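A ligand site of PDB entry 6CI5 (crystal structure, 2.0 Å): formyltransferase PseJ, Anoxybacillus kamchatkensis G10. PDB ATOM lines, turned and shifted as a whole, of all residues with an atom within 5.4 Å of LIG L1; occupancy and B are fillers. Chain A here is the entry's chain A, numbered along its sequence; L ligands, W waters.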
ATOM      1  N   ARG A  35      20.642   3.980  -9.923  1.00  0.00           N
ATOM      2  CA  ARG A  35      19.750   4.245  -8.790  1.00  0.00           C
ATOM      3  C   ARG A  35      20.002   3.146  -7.761  1.00  0.00           C
ATOM      4  O   ARG A  35      19.541   2.013  -7.925  1.00  0.00           O
ATOM      5  CB  ARG A  35      18.298   4.277  -9.231  1.00  0.00           C
ATOM      6  CG  ARG A  35      17.999   5.219 -10.383  1.00  0.00           C
ATOM      7  CD  ARG A  35      16.533   5.096 -10.814  1.00  0.00           C
ATOM      8  NE  ARG A  35      16.303   5.648 -12.151  1.00  0.00           N
ATOM      9  CZ  ARG A  35      15.852   6.878 -12.394  1.00  0.00           C
ATOM     10  NH1 ARG A  35      15.568   7.713 -11.409  1.00  0.00           N
ATOM     11  NH2 ARG A  35      15.668   7.268 -13.649  1.00  0.00           N
ATOM     12  N   TYR A  72      14.245   2.992 -17.482  1.00  0.00           N
ATOM     13  CA  TYR A  72      13.733   4.054 -16.616  1.00  0.00           C
ATOM     14  C   TYR A  72      14.689   5.242 -16.742  1.00  0.00           C
ATOM     15  O   TYR A  72      15.775   5.226 -16.170  1.00  0.00           O
ATOM     16  CB  TYR A  72      13.629   3.564 -15.167  1.00  0.00           C
ATOM     17  CG  TYR A  72      13.047   4.585 -14.208  1.00  0.00           C
ATOM     18  CD1 TYR A  72      12.192   5.588 -14.652  1.00  0.00           C
ATOM     19  CD2 TYR A  72      13.349   4.537 -12.854  1.00  0.00           C
ATOM     20  CE1 TYR A  72      11.650   6.502 -13.776  1.00  0.00           C
ATOM     21  CE2 TYR A  72      12.823   5.454 -11.965  1.00  0.00           C
ATOM     22  CZ  TYR A  72      11.969   6.436 -12.437  1.00  0.00           C
ATOM     23  OH  TYR A  72      11.449   7.354 -11.556  1.00  0.00           O
ATOM     24  N   GLY A  73      14.264   6.256 -17.495  1.00  0.00           N
ATOM     25  CA  GLY A  73      15.124   7.380 -17.757  1.00  0.00           C
ATOM     26  C   GLY A  73      16.129   7.148 -18.859  1.00  0.00           C
ATOM     27  O   GLY A  73      17.005   7.992 -19.066  1.00  0.00           O
ATOM     28  N   TYR A  74      16.048   6.018 -19.569  1.00  0.00           N
ATOM     29  CA  TYR A  74      16.959   5.749 -20.660  1.00  0.00           C
ATOM     30  C   TYR A  74      16.717   6.743 -21.798  1.00  0.00           C
ATOM     31  O   TYR A  74      15.572   6.958 -22.212  1.00  0.00           O
ATOM     32  CB  TYR A  74      16.785   4.313 -21.146  1.00  0.00           C
ATOM     33  CG  TYR A  74      17.843   3.861 -22.128  1.00  0.00           C
ATOM     34  CD1 TYR A  74      19.192   3.958 -21.820  1.00  0.00           C
ATOM     35  CD2 TYR A  74      17.489   3.323 -23.362  1.00  0.00           C
ATOM     36  CE1 TYR A  74      20.166   3.544 -22.710  1.00  0.00           C
ATOM     37  CE2 TYR A  74      18.449   2.907 -24.251  1.00  0.00           C
ATOM     38  CZ  TYR A  74      19.782   3.021 -23.929  1.00  0.00           C
ATOM     39  OH  TYR A  74      20.741   2.604 -24.818  1.00  0.00           O
ATOM     40  N   ARG A  75      17.791   7.340 -22.302  1.00  0.00           N
ATOM     41  CA  ARG A  75      17.697   8.462 -23.225  1.00  0.00           C
ATOM     42  C   ARG A  75      18.042   8.062 -24.664  1.00  0.00           C
ATOM     43  O   ARG A  75      18.557   8.878 -25.428  1.00  0.00           O
ATOM     44  CB  ARG A  75      18.613   9.591 -22.768  1.00  0.00           C
ATOM     45  CG  ARG A  75      18.434   9.974 -21.300  1.00  0.00           C
ATOM     46  CD  ARG A  75      19.057  11.316 -20.991  1.00  0.00           C
ATOM     47  NE  ARG A  75      18.417  12.401 -21.729  1.00  0.00           N
ATOM     48  CZ  ARG A  75      17.254  12.953 -21.404  1.00  0.00           C
ATOM     49  NH1 ARG A  75      16.757  13.932 -22.142  1.00  0.00           N
ATOM     50  NH2 ARG A  75      16.579  12.523 -20.348  1.00  0.00           N
ATOM     51  N   TYR A  76      17.761   6.823 -25.045  1.00  0.00           N
ATOM     52  CA  TYR A  76      18.019   6.358 -26.395  1.00  0.00           C
ATOM     53  C   TYR A  76      16.942   5.372 -26.809  1.00  0.00           C
ATOM     54  O   TYR A  76      16.342   4.694 -25.982  1.00  0.00           O
ATOM     55  CB  TYR A  76      19.397   5.691 -26.519  1.00  0.00           C
ATOM     56  CG  TYR A  76      20.545   6.560 -26.048  1.00  0.00           C
ATOM     57  CD1 TYR A  76      21.073   7.539 -26.885  1.00  0.00           C
ATOM     58  CD2 TYR A  76      21.105   6.394 -24.796  1.00  0.00           C
ATOM     59  CE1 TYR A  76      22.121   8.336 -26.465  1.00  0.00           C
ATOM     60  CE2 TYR A  76      22.149   7.180 -24.368  1.00  0.00           C
ATOM     61  CZ  TYR A  76      22.663   8.157 -25.203  1.00  0.00           C
ATOM     62  OH  TYR A  76      23.699   8.941 -24.782  1.00  0.00           O
ATOM     63  N   ASN A  92       9.215  -0.450 -19.862  1.00  0.00           N
ATOM     64  CA  ASN A  92       9.688   0.920 -19.698  1.00  0.00           C
ATOM     65  C   ASN A  92       8.797   1.619 -18.680  1.00  0.00           C
ATOM     66  O   ASN A  92       7.567   1.483 -18.727  1.00  0.00           O
ATOM     67  CB  ASN A  92       9.666   1.675 -21.036  1.00  0.00           C
ATOM     68  CG  ASN A  92      10.109   3.121 -20.886  1.00  0.00           C
ATOM     69  OD1 ASN A  92      11.268   3.395 -20.556  1.00  0.00           O
ATOM     70  ND2 ASN A  92       9.193   4.046 -21.143  1.00  0.00           N
ATOM     71  N   LEU A  93       9.428   2.353 -17.765  1.00  0.00           N
ATOM     72  CA  LEU A  93       8.702   3.153 -16.781  1.00  0.00           C
ATOM     73  C   LEU A  93       8.589   4.569 -17.349  1.00  0.00           C
ATOM     74  O   LEU A  93       9.578   5.307 -17.411  1.00  0.00           O
ATOM     75  CB  LEU A  93       9.428   3.155 -15.439  1.00  0.00           C
ATOM     76  CG  LEU A  93       9.984   1.823 -14.916  1.00  0.00           C
ATOM     77  CD1 LEU A  93      10.331   1.950 -13.439  1.00  0.00           C
ATOM     78  CD2 LEU A  93       9.024   0.663 -15.140  1.00  0.00           C
ATOM     79  N   HIS A  94       7.380   4.934 -17.757  1.00  0.00           N
ATOM     80  CA  HIS A  94       7.124   6.196 -18.446  1.00  0.00           C
ATOM     81  C   HIS A  94       6.211   7.049 -17.569  1.00  0.00           C
ATOM     82  O   HIS A  94       5.116   6.607 -17.207  1.00  0.00           O
ATOM     83  CB  HIS A  94       6.499   5.958 -19.813  1.00  0.00           C
ATOM     84  CG  HIS A  94       6.400   7.184 -20.664  1.00  0.00           C
ATOM     85  ND1 HIS A  94       7.513   7.871 -21.111  1.00  0.00           N
ATOM     86  CD2 HIS A  94       5.329   7.848 -21.156  1.00  0.00           C
ATOM     87  CE1 HIS A  94       7.122   8.913 -21.833  1.00  0.00           C
ATOM     88  NE2 HIS A  94       5.802   8.912 -21.872  1.00  0.00           N
ATOM     89  N   ILE A  95       6.666   8.258 -17.245  1.00  0.00           N
ATOM     90  CA  ILE A  95       5.908   9.112 -16.333  1.00  0.00           C
ATOM     91  C   ILE A  95       4.847   9.890 -17.102  1.00  0.00           C
ATOM     92  O   ILE A  95       4.789  11.115 -17.025  1.00  0.00           O
ATOM     93  CB  ILE A  95       6.845  10.072 -15.556  1.00  0.00           C
ATOM     94  CG1 ILE A  95       7.780  10.820 -16.517  1.00  0.00           C
ATOM     95  CG2 ILE A  95       7.651   9.294 -14.529  1.00  0.00           C
ATOM     96  CD1 ILE A  95       8.488  11.997 -15.887  1.00  0.00           C
ATOM     97  N   GLY A 103       6.803   9.947 -25.554  1.00  0.00           N
ATOM     98  CA  GLY A 103       8.064  10.585 -25.913  1.00  0.00           C
ATOM     99  C   GLY A 103       8.586  11.497 -24.820  1.00  0.00           C
ATOM    100  O   GLY A 103       8.584  11.129 -23.649  1.00  0.00           O
ATOM    101  N   ALA A 104       9.002  12.694 -25.203  1.00  0.00           N
ATOM    102  CA  ALA A 104       9.819  13.552 -24.367  1.00  0.00           C
ATOM    103  C   ALA A 104       8.983  14.540 -23.554  1.00  0.00           C
ATOM    104  O   ALA A 104       7.922  14.994 -23.987  1.00  0.00           O
ATOM    105  CB  ALA A 104      10.827  14.318 -25.215  1.00  0.00           C
ATOM    106  N   ASP A 105       9.493  14.872 -22.373  1.00  0.00           N
ATOM    107  CA  ASP A 105       8.910  15.890 -21.505  1.00  0.00           C
ATOM    108  C   ASP A 105       7.424  15.665 -21.240  1.00  0.00           C
ATOM    109  O   ASP A 105       6.622  16.607 -21.338  1.00  0.00           O
ATOM    110  CB  ASP A 105       9.139  17.269 -22.109  1.00  0.00           C
ATOM    111  CG  ASP A 105      10.606  17.551 -22.382  1.00  0.00           C
ATOM    112  OD1 ASP A 105      11.440  17.325 -21.471  1.00  0.00           O
ATOM    113  OD2 ASP A 105      10.932  17.994 -23.500  1.00  0.00           O
ATOM    114  N   PRO A 106       7.025  14.449 -20.872  1.00  0.00           N
ATOM    115  CA  PRO A 106       5.582  14.189 -20.680  1.00  0.00           C
ATOM    116  C   PRO A 106       4.950  15.041 -19.601  1.00  0.00           C
ATOM    117  O   PRO A 106       3.822  15.522 -19.773  1.00  0.00           O
ATOM    118  CB  PRO A 106       5.536  12.694 -20.343  1.00  0.00           C
ATOM    119  CG  PRO A 106       6.904  12.383 -19.824  1.00  0.00           C
ATOM    120  CD  PRO A 106       7.843  13.261 -20.571  1.00  0.00           C
ATOM    121  N   ASN A 107       5.641  15.263 -18.480  1.00  0.00           N
ATOM    122  CA  ASN A 107       5.075  16.067 -17.404  1.00  0.00           C
ATOM    123  C   ASN A 107       4.712  17.458 -17.905  1.00  0.00           C
ATOM    124  O   ASN A 107       3.580  17.930 -17.707  1.00  0.00           O
ATOM    125  CB  ASN A 107       6.061  16.164 -16.239  1.00  0.00           C
ATOM    126  CG  ASN A 107       5.463  16.865 -15.034  1.00  0.00           C
ATOM    127  OD1 ASN A 107       4.321  16.608 -14.649  1.00  0.00           O
ATOM    128  ND2 ASN A 107       6.241  17.769 -14.432  1.00  0.00           N
ATOM    129  N   LEU A 108       5.656  18.127 -18.557  1.00  0.00           N
ATOM    130  CA  LEU A 108       5.388  19.452 -19.106  1.00  0.00           C
ATOM    131  C   LEU A 108       4.212  19.427 -20.080  1.00  0.00           C
ATOM    132  O   LEU A 108       3.299  20.254 -19.984  1.00  0.00           O
ATOM    133  CB  LEU A 108       6.650  19.987 -19.800  1.00  0.00           C
ATOM    134  CG  LEU A 108       6.505  21.319 -20.545  1.00  0.00           C
ATOM    135  CD1 LEU A 108       6.108  22.427 -19.593  1.00  0.00           C
ATOM    136  CD2 LEU A 108       7.793  21.654 -21.282  1.00  0.00           C
ATOM    137  N   HIS A 122       4.783  -0.110 -19.285  1.00  0.00           N
ATOM    138  CA  HIS A 122       4.355  -0.724 -20.537  1.00  0.00           C
ATOM    139  C   HIS A 122       5.487  -1.545 -21.115  1.00  0.00           C
ATOM    140  O   HIS A 122       6.669  -1.211 -20.953  1.00  0.00           O
ATOM    141  CB  HIS A 122       3.903   0.336 -21.553  1.00  0.00           C
ATOM    142  CG  HIS A 122       5.012   1.204 -22.059  1.00  0.00           C
ATOM    143  ND1 HIS A 122       5.767   0.873 -23.169  1.00  0.00           N
ATOM    144  CD2 HIS A 122       5.508   2.375 -21.602  1.00  0.00           C
ATOM    145  CE1 HIS A 122       6.667   1.813 -23.383  1.00  0.00           C
ATOM    146  NE2 HIS A 122       6.535   2.737 -22.445  1.00  0.00           N
ATOM    147  N   ASP A 129       7.236   4.481 -26.933  1.00  0.00           N
ATOM    148  CA  ASP A 129       6.186   4.488 -25.909  1.00  0.00           C
ATOM    149  C   ASP A 129       4.834   4.076 -26.477  1.00  0.00           C
ATOM    150  O   ASP A 129       3.799   4.624 -26.100  1.00  0.00           O
ATOM    151  CB  ASP A 129       6.087   5.867 -25.238  1.00  0.00           C
ATOM    152  CG  ASP A 129       7.403   6.323 -24.654  1.00  0.00           C
ATOM    153  OD1 ASP A 129       8.171   5.458 -24.174  1.00  0.00           O
ATOM    154  OD2 ASP A 129       7.677   7.547 -24.671  1.00  0.00           O
ATOM    155  N   LEU A 147       6.362  22.304 -11.797  1.00  0.00           N
ATOM    156  CA  LEU A 147       6.869  21.192 -12.596  1.00  0.00           C
ATOM    157  C   LEU A 147       7.784  20.306 -11.765  1.00  0.00           C
ATOM    158  O   LEU A 147       7.853  19.088 -12.000  1.00  0.00           O
ATOM    159  CB  LEU A 147       7.604  21.709 -13.825  1.00  0.00           C
ATOM    160  CG  LEU A 147       6.742  22.372 -14.912  1.00  0.00           C
ATOM    161  CD1 LEU A 147       7.618  22.931 -16.022  1.00  0.00           C
ATOM    162  CD2 LEU A 147       5.718  21.402 -15.489  1.00  0.00           C
ATOM    163  N   ARG A 148       8.488  20.882 -10.784  1.00  0.00           N
ATOM    164  CA  ARG A 148       9.351  20.089  -9.932  1.00  0.00           C
ATOM    165  C   ARG A 148       8.551  19.182  -9.010  1.00  0.00           C
ATOM    166  O   ARG A 148       8.793  17.978  -8.935  1.00  0.00           O
ATOM    167  CB  ARG A 148      10.273  20.997  -9.108  1.00  0.00           C
ATOM    168  CG  ARG A 148      11.262  20.239  -8.241  1.00  0.00           C
ATOM    169  CD  ARG A 148      12.090  21.171  -7.375  1.00  0.00           C
ATOM    170  NE  ARG A 148      12.839  22.144  -8.174  1.00  0.00           N
ATOM    171  CZ  ARG A 148      13.946  21.854  -8.862  1.00  0.00           C
ATOM    172  NH1 ARG A 148      14.560  22.794  -9.556  1.00  0.00           N
ATOM    173  NH2 ARG A 148      14.426  20.611  -8.870  1.00  0.00           N
ATOM    174  N   TYR A 151       6.734  16.541 -11.072  1.00  0.00           N
ATOM    175  CA  TYR A 151       7.696  15.539 -11.512  1.00  0.00           C
ATOM    176  C   TYR A 151       8.078  14.613 -10.369  1.00  0.00           C
ATOM    177  O   TYR A 151       8.099  13.389 -10.528  1.00  0.00           O
ATOM    178  CB  TYR A 151       8.933  16.226 -12.092  1.00  0.00           C
ATOM    179  CG  TYR A 151       9.961  15.274 -12.654  1.00  0.00           C
ATOM    180  CD1 TYR A 151      10.027  15.015 -14.018  1.00  0.00           C
ATOM    181  CD2 TYR A 151      10.880  14.633 -11.829  1.00  0.00           C
ATOM    182  CE1 TYR A 151      10.963  14.148 -14.541  1.00  0.00           C
ATOM    183  CE2 TYR A 151      11.824  13.767 -12.345  1.00  0.00           C
ATOM    184  CZ  TYR A 151      11.851  13.522 -13.700  1.00  0.00           C
ATOM    185  OH  TYR A 151      12.787  12.655 -14.222  1.00  0.00           O
ATOM    186  N   GLU A 152       8.368  15.187  -9.194  1.00  0.00           N
ATOM    187  CA  GLU A 152       8.732  14.359  -8.054  1.00  0.00           C
ATOM    188  C   GLU A 152       7.586  13.439  -7.648  1.00  0.00           C
ATOM    189  O   GLU A 152       7.812  12.283  -7.282  1.00  0.00           O
ATOM    190  CB  GLU A 152       9.145  15.243  -6.871  1.00  0.00           C
ATOM    191  CG  GLU A 152      10.427  16.032  -7.090  1.00  0.00           C
ATOM    192  CD  GLU A 152      11.634  15.145  -7.330  1.00  0.00           C
ATOM    193  OE1 GLU A 152      12.346  15.359  -8.343  1.00  0.00           O
ATOM    194  OE2 GLU A 152      11.874  14.220  -6.522  1.00  0.00           O
ATOM    195  N   LEU A 188      11.747  16.216 -28.223  1.00  0.00           N
ATOM    196  CA  LEU A 188      12.434  17.143 -27.330  1.00  0.00           C
ATOM    197  C   LEU A 188      12.345  18.575 -27.836  1.00  0.00           C
ATOM    198  O   LEU A 188      12.147  19.502 -27.042  1.00  0.00           O
ATOM    199  CB  LEU A 188      13.897  16.727 -27.148  1.00  0.00           C
ATOM    200  CG  LEU A 188      14.234  15.834 -25.960  1.00  0.00           C
ATOM    201  CD1 LEU A 188      15.682  15.407 -26.024  1.00  0.00           C
ATOM    202  CD2 LEU A 188      13.942  16.546 -24.634  1.00  0.00           C
ATOM    203  N   TRP A 202      12.286  24.371 -13.520  1.00  0.00           N
ATOM    204  CA  TRP A 202      11.412  23.346 -12.985  1.00  0.00           C
ATOM    205  C   TRP A 202      10.584  23.838 -11.798  1.00  0.00           C
ATOM    206  O   TRP A 202       9.618  23.176 -11.422  1.00  0.00           O
ATOM    207  CB  TRP A 202      12.213  22.118 -12.574  1.00  0.00           C
ATOM    208  CG  TRP A 202      13.008  21.529 -13.695  1.00  0.00           C
ATOM    209  CD1 TRP A 202      14.341  21.215 -13.684  1.00  0.00           C
ATOM    210  CD2 TRP A 202      12.536  21.190 -15.015  1.00  0.00           C
ATOM    211  NE1 TRP A 202      14.723  20.697 -14.900  1.00  0.00           N
ATOM    212  CE2 TRP A 202      13.624  20.681 -15.733  1.00  0.00           C
ATOM    213  CE3 TRP A 202      11.294  21.276 -15.640  1.00  0.00           C
ATOM    214  CZ2 TRP A 202      13.517  20.249 -17.051  1.00  0.00           C
ATOM    215  CZ3 TRP A 202      11.179  20.852 -16.952  1.00  0.00           C
ATOM    216  CH2 TRP A 202      12.283  20.348 -17.643  1.00  0.00           C
HETATM  217  C1  LIG L   1      15.875  15.560 -15.174  1.00  0.00           C
HETATM  218  C2  LIG L   1      14.775  15.560 -13.142  1.00  0.00           C
HETATM  219  C3  LIG L   1      11.514  18.545 -13.010  1.00  0.00           C
HETATM  220  C4  LIG L   1      11.168  17.718 -15.880  1.00  0.00           C
HETATM  221  C5  LIG L   1      11.561   9.638 -21.393  1.00  0.00           C
HETATM  222  C6  LIG L   1      10.533   7.286 -21.223  1.00  0.00           C
HETATM  223  C7  LIG L   1      11.167   9.857 -19.926  1.00  0.00           C
HETATM  224  C8  LIG L   1       9.709  10.161 -19.833  1.00  0.00           C
HETATM  225  C9  LIG L   1      13.392  10.729 -19.445  1.00  0.00           C
HETATM  226  C10 LIG L   1      15.607  16.256 -13.856  1.00  0.00           C
HETATM  227  C11 LIG L   1      14.047  16.600 -12.312  1.00  0.00           C
HETATM  228  C12 LIG L   1      14.000  17.864 -13.219  1.00  0.00           C
HETATM  229  C13 LIG L   1      10.038  18.240 -15.130  1.00  0.00           C
HETATM  230  C14 LIG L   1      12.468  17.603 -15.237  1.00  0.00           C
HETATM  231  C15 LIG L   1      13.815  10.486 -20.892  1.00  0.00           C
HETATM  232  C16 LIG L   1      14.313  12.011 -22.891  1.00  0.00           C
HETATM  233  C17 LIG L   1      15.329  11.016 -23.429  1.00  0.00           C
HETATM  234  C18 LIG L   1      13.029   9.386 -21.512  1.00  0.00           C
HETATM  235  N1  LIG L   1      10.793   8.503 -21.977  1.00  0.00           N
HETATM  236  N2  LIG L   1      12.656  17.992 -13.845  1.00  0.00           N
HETATM  237  N3  LIG L   1      10.179  18.640 -13.749  1.00  0.00           N
HETATM  238  N4  LIG L   1      13.581  11.739 -21.668  1.00  0.00           N
HETATM  239  O1  LIG L   1       9.912   6.406 -21.720  1.00  0.00           O
HETATM  240  O2  LIG L   1      11.941  10.974 -19.328  1.00  0.00           O
HETATM  241  O3  LIG L   1      14.047  11.820 -18.934  1.00  0.00           O
HETATM  242  O4  LIG L   1      14.832  10.731 -16.730  1.00  0.00           O
HETATM  243  O5  LIG L   1      14.961  13.309 -16.867  1.00  0.00           O
HETATM  244  O6  LIG L   1      14.815  15.856 -16.039  1.00  0.00           O
HETATM  245  O7  LIG L   1       8.984  18.335 -15.666  1.00  0.00           O
HETATM  246  O8  LIG L   1      11.645  18.863 -11.880  1.00  0.00           O
HETATM  247  O9  LIG L   1      14.891  17.689 -14.121  1.00  0.00           O
HETATM  248  O10 LIG L   1      14.733  16.863 -11.164  1.00  0.00           O
HETATM  249  O11 LIG L   1      15.509  14.601 -12.234  1.00  0.00           O
HETATM  250  O12 LIG L   1      13.008  14.845 -17.596  1.00  0.00           O
HETATM  251  O13 LIG L   1      15.251  15.275 -18.515  1.00  0.00           O
HETATM  252  O14 LIG L   1      12.733  12.009 -16.729  1.00  0.00           O
HETATM  253  O15 LIG L   1      14.107  13.021 -23.479  1.00  0.00           O
HETATM  254  O16 LIG L   1      13.340   8.135 -20.828  1.00  0.00           O
HETATM  255  P1  LIG L   1      14.136  11.944 -17.292  1.00  0.00           P
HETATM  256  P2  LIG L   1      14.495  14.825 -17.294  1.00  0.00           P
HETATM  257  N1  LG2 L   2      10.394   1.832 -27.108  1.00  0.00           N
HETATM  258  C1  LG2 L   2      11.823   1.804 -27.619  1.00  0.00           C
HETATM  259  N2  LG2 L   2      12.918   2.439 -26.818  1.00  0.00           N
HETATM  260  C2  LG2 L   2      12.612   3.086 -25.537  1.00  0.00           C
HETATM  261  C3  LG2 L   2      11.176   3.113 -25.019  1.00  0.00           C
HETATM  262  C4  LG2 L   2      10.082   2.468 -25.833  1.00  0.00           C
HETATM  263  N3  LG2 L   2      13.635   3.663 -24.841  1.00  0.00           N
HETATM  264  C5  LG2 L   2      13.247   4.328 -23.468  1.00  0.00           C
HETATM  265  C6  LG2 L   2      11.940   4.764 -23.352  1.00  0.00           C
HETATM  266  N4  LG2 L   2      10.870   3.706 -23.835  1.00  0.00           N
HETATM  267  C7  LG2 L   2      11.778   6.050 -24.143  1.00  0.00           C
HETATM  268  O1  LG2 L   2       8.962   2.480 -25.435  1.00  0.00           O
HETATM  269  N5  LG2 L   2      12.129   1.167 -28.886  1.00  0.00           N
HETATM  270  O   HOH W   1      14.151   9.279 -14.846  1.00  0.00           O
HETATM  271  O   HOH W   2      11.864   9.515 -15.955  1.00  0.00           O
HETATM  272  O   HOH W   3      10.847  13.408 -18.573  1.00  0.00           O
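N of Gly 103 is in hydrogen-bond range of OD2 of Asp 129, 2.7 Å away. The side-chain carboxylate (OD1) of Asp 129 is in hydrogen-bond range of the side-chain amide nitrogen (ND2) of Asn 92, at 3.5 Å. The backbone NH (N) of Asn 92 lies within hydrogen-bond range of the backbone carbonyl oxygen (O) of His 122 (2.9 Å). The backbone NH of Arg 148 lies within hydrogen-bond range of the backbone carbonyl oxygen of Trp 202, at 2.6 Å. The side-chain amide nitrogen (ND2) of Asn 107 lies within hydrogen-bond range of the backbone carbonyl oxygen (O) of Leu 147, 3.2 Å away. The backbone NH (N) of Leu 147 lies within hydrogen-bond range of the backbone carbonyl oxygen (O) of Trp 202, at 3.4 Å.
The side-chain carboxylate (OD1) of Asp 129 lies close to an oxygen (O1) of LIG L1 (3.2 Å). Merely in contact with LIG L1: Arg 148, Gly 73, Pro 106, Leu 188, Gly 103, Ile 95, Ala 104 and Glu 152. Hydrophobic or aromatic side chains within 4 Å of LIG L1: His 94, Ile 95, Ala 104, Pro 106, Tyr 151, Leu 188 and Trp 202. Within 4 Å of LIG L1: Gly 73, Tyr 74, Arg 75, Asn 92, His 94, Ile 95, Gly 103, Ala 104, Pro 106, Asn 107, Asp 129, Leu 147, Arg 148, Tyr 151, Glu 152, Leu 188 and Trp 202. The nearest printed residue that does not touch LIG L1 is Leu 93 (4.4 Å).
Water W1 bridges O4 of LIG L1 and NH2 of Arg 35.
ND2 of Asn 92 lies close to N4 of LG2 L2 (3.2 Å). The backbone carbonyl oxygen (O) of Tyr 74 lies within hydrogen-bond range of an oxygen (O16) of LIG L1 (2.9 Å). The side-chain amide nitrogen of Asn 92 sits at hydrogen-bond distance from an oxygen (O1) of LIG L1 (2.5 Å). O14 of LIG L1 is in hydrogen-bond range of OH of Tyr 151, 2.6 Å away. The backbone NH of Asp 129 lies within hydrogen-bond range of an oxygen (O1) of LG2 L2 (3.0 Å). An oxygen (O13) of LIG L1 is in salt-bridge range of the guanidinium group (NH2) of Arg 75, at 3.6 Å. An oxygen (O7) of LIG L1 sits at hydrogen-bond distance from the side-chain amide nitrogen of Asn 107 (3.1 Å). O9 of LIG L1 is in hydrogen-bond range of NE1 of Trp 202 (3.1 Å). A ring nitrogen (ND1) of His 94 lies within hydrogen-bond range of an oxygen (O1) of LIG L1, at 2.9 Å. The backbone carbonyl oxygen (O) of Leu 147 is in hydrogen-bond range of a nitrogen (N3) of LIG L1. The backbone carbonyl oxygen (O) of Tyr 76 lies within hydrogen-bond range of a nitrogen (N3) of LG2 L2 (3.1 Å). The side-chain carboxylate (OD1) of Asp 129 lies within hydrogen-bond range of a nitrogen (N4) of LG2 L2, 3.2 Å away.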
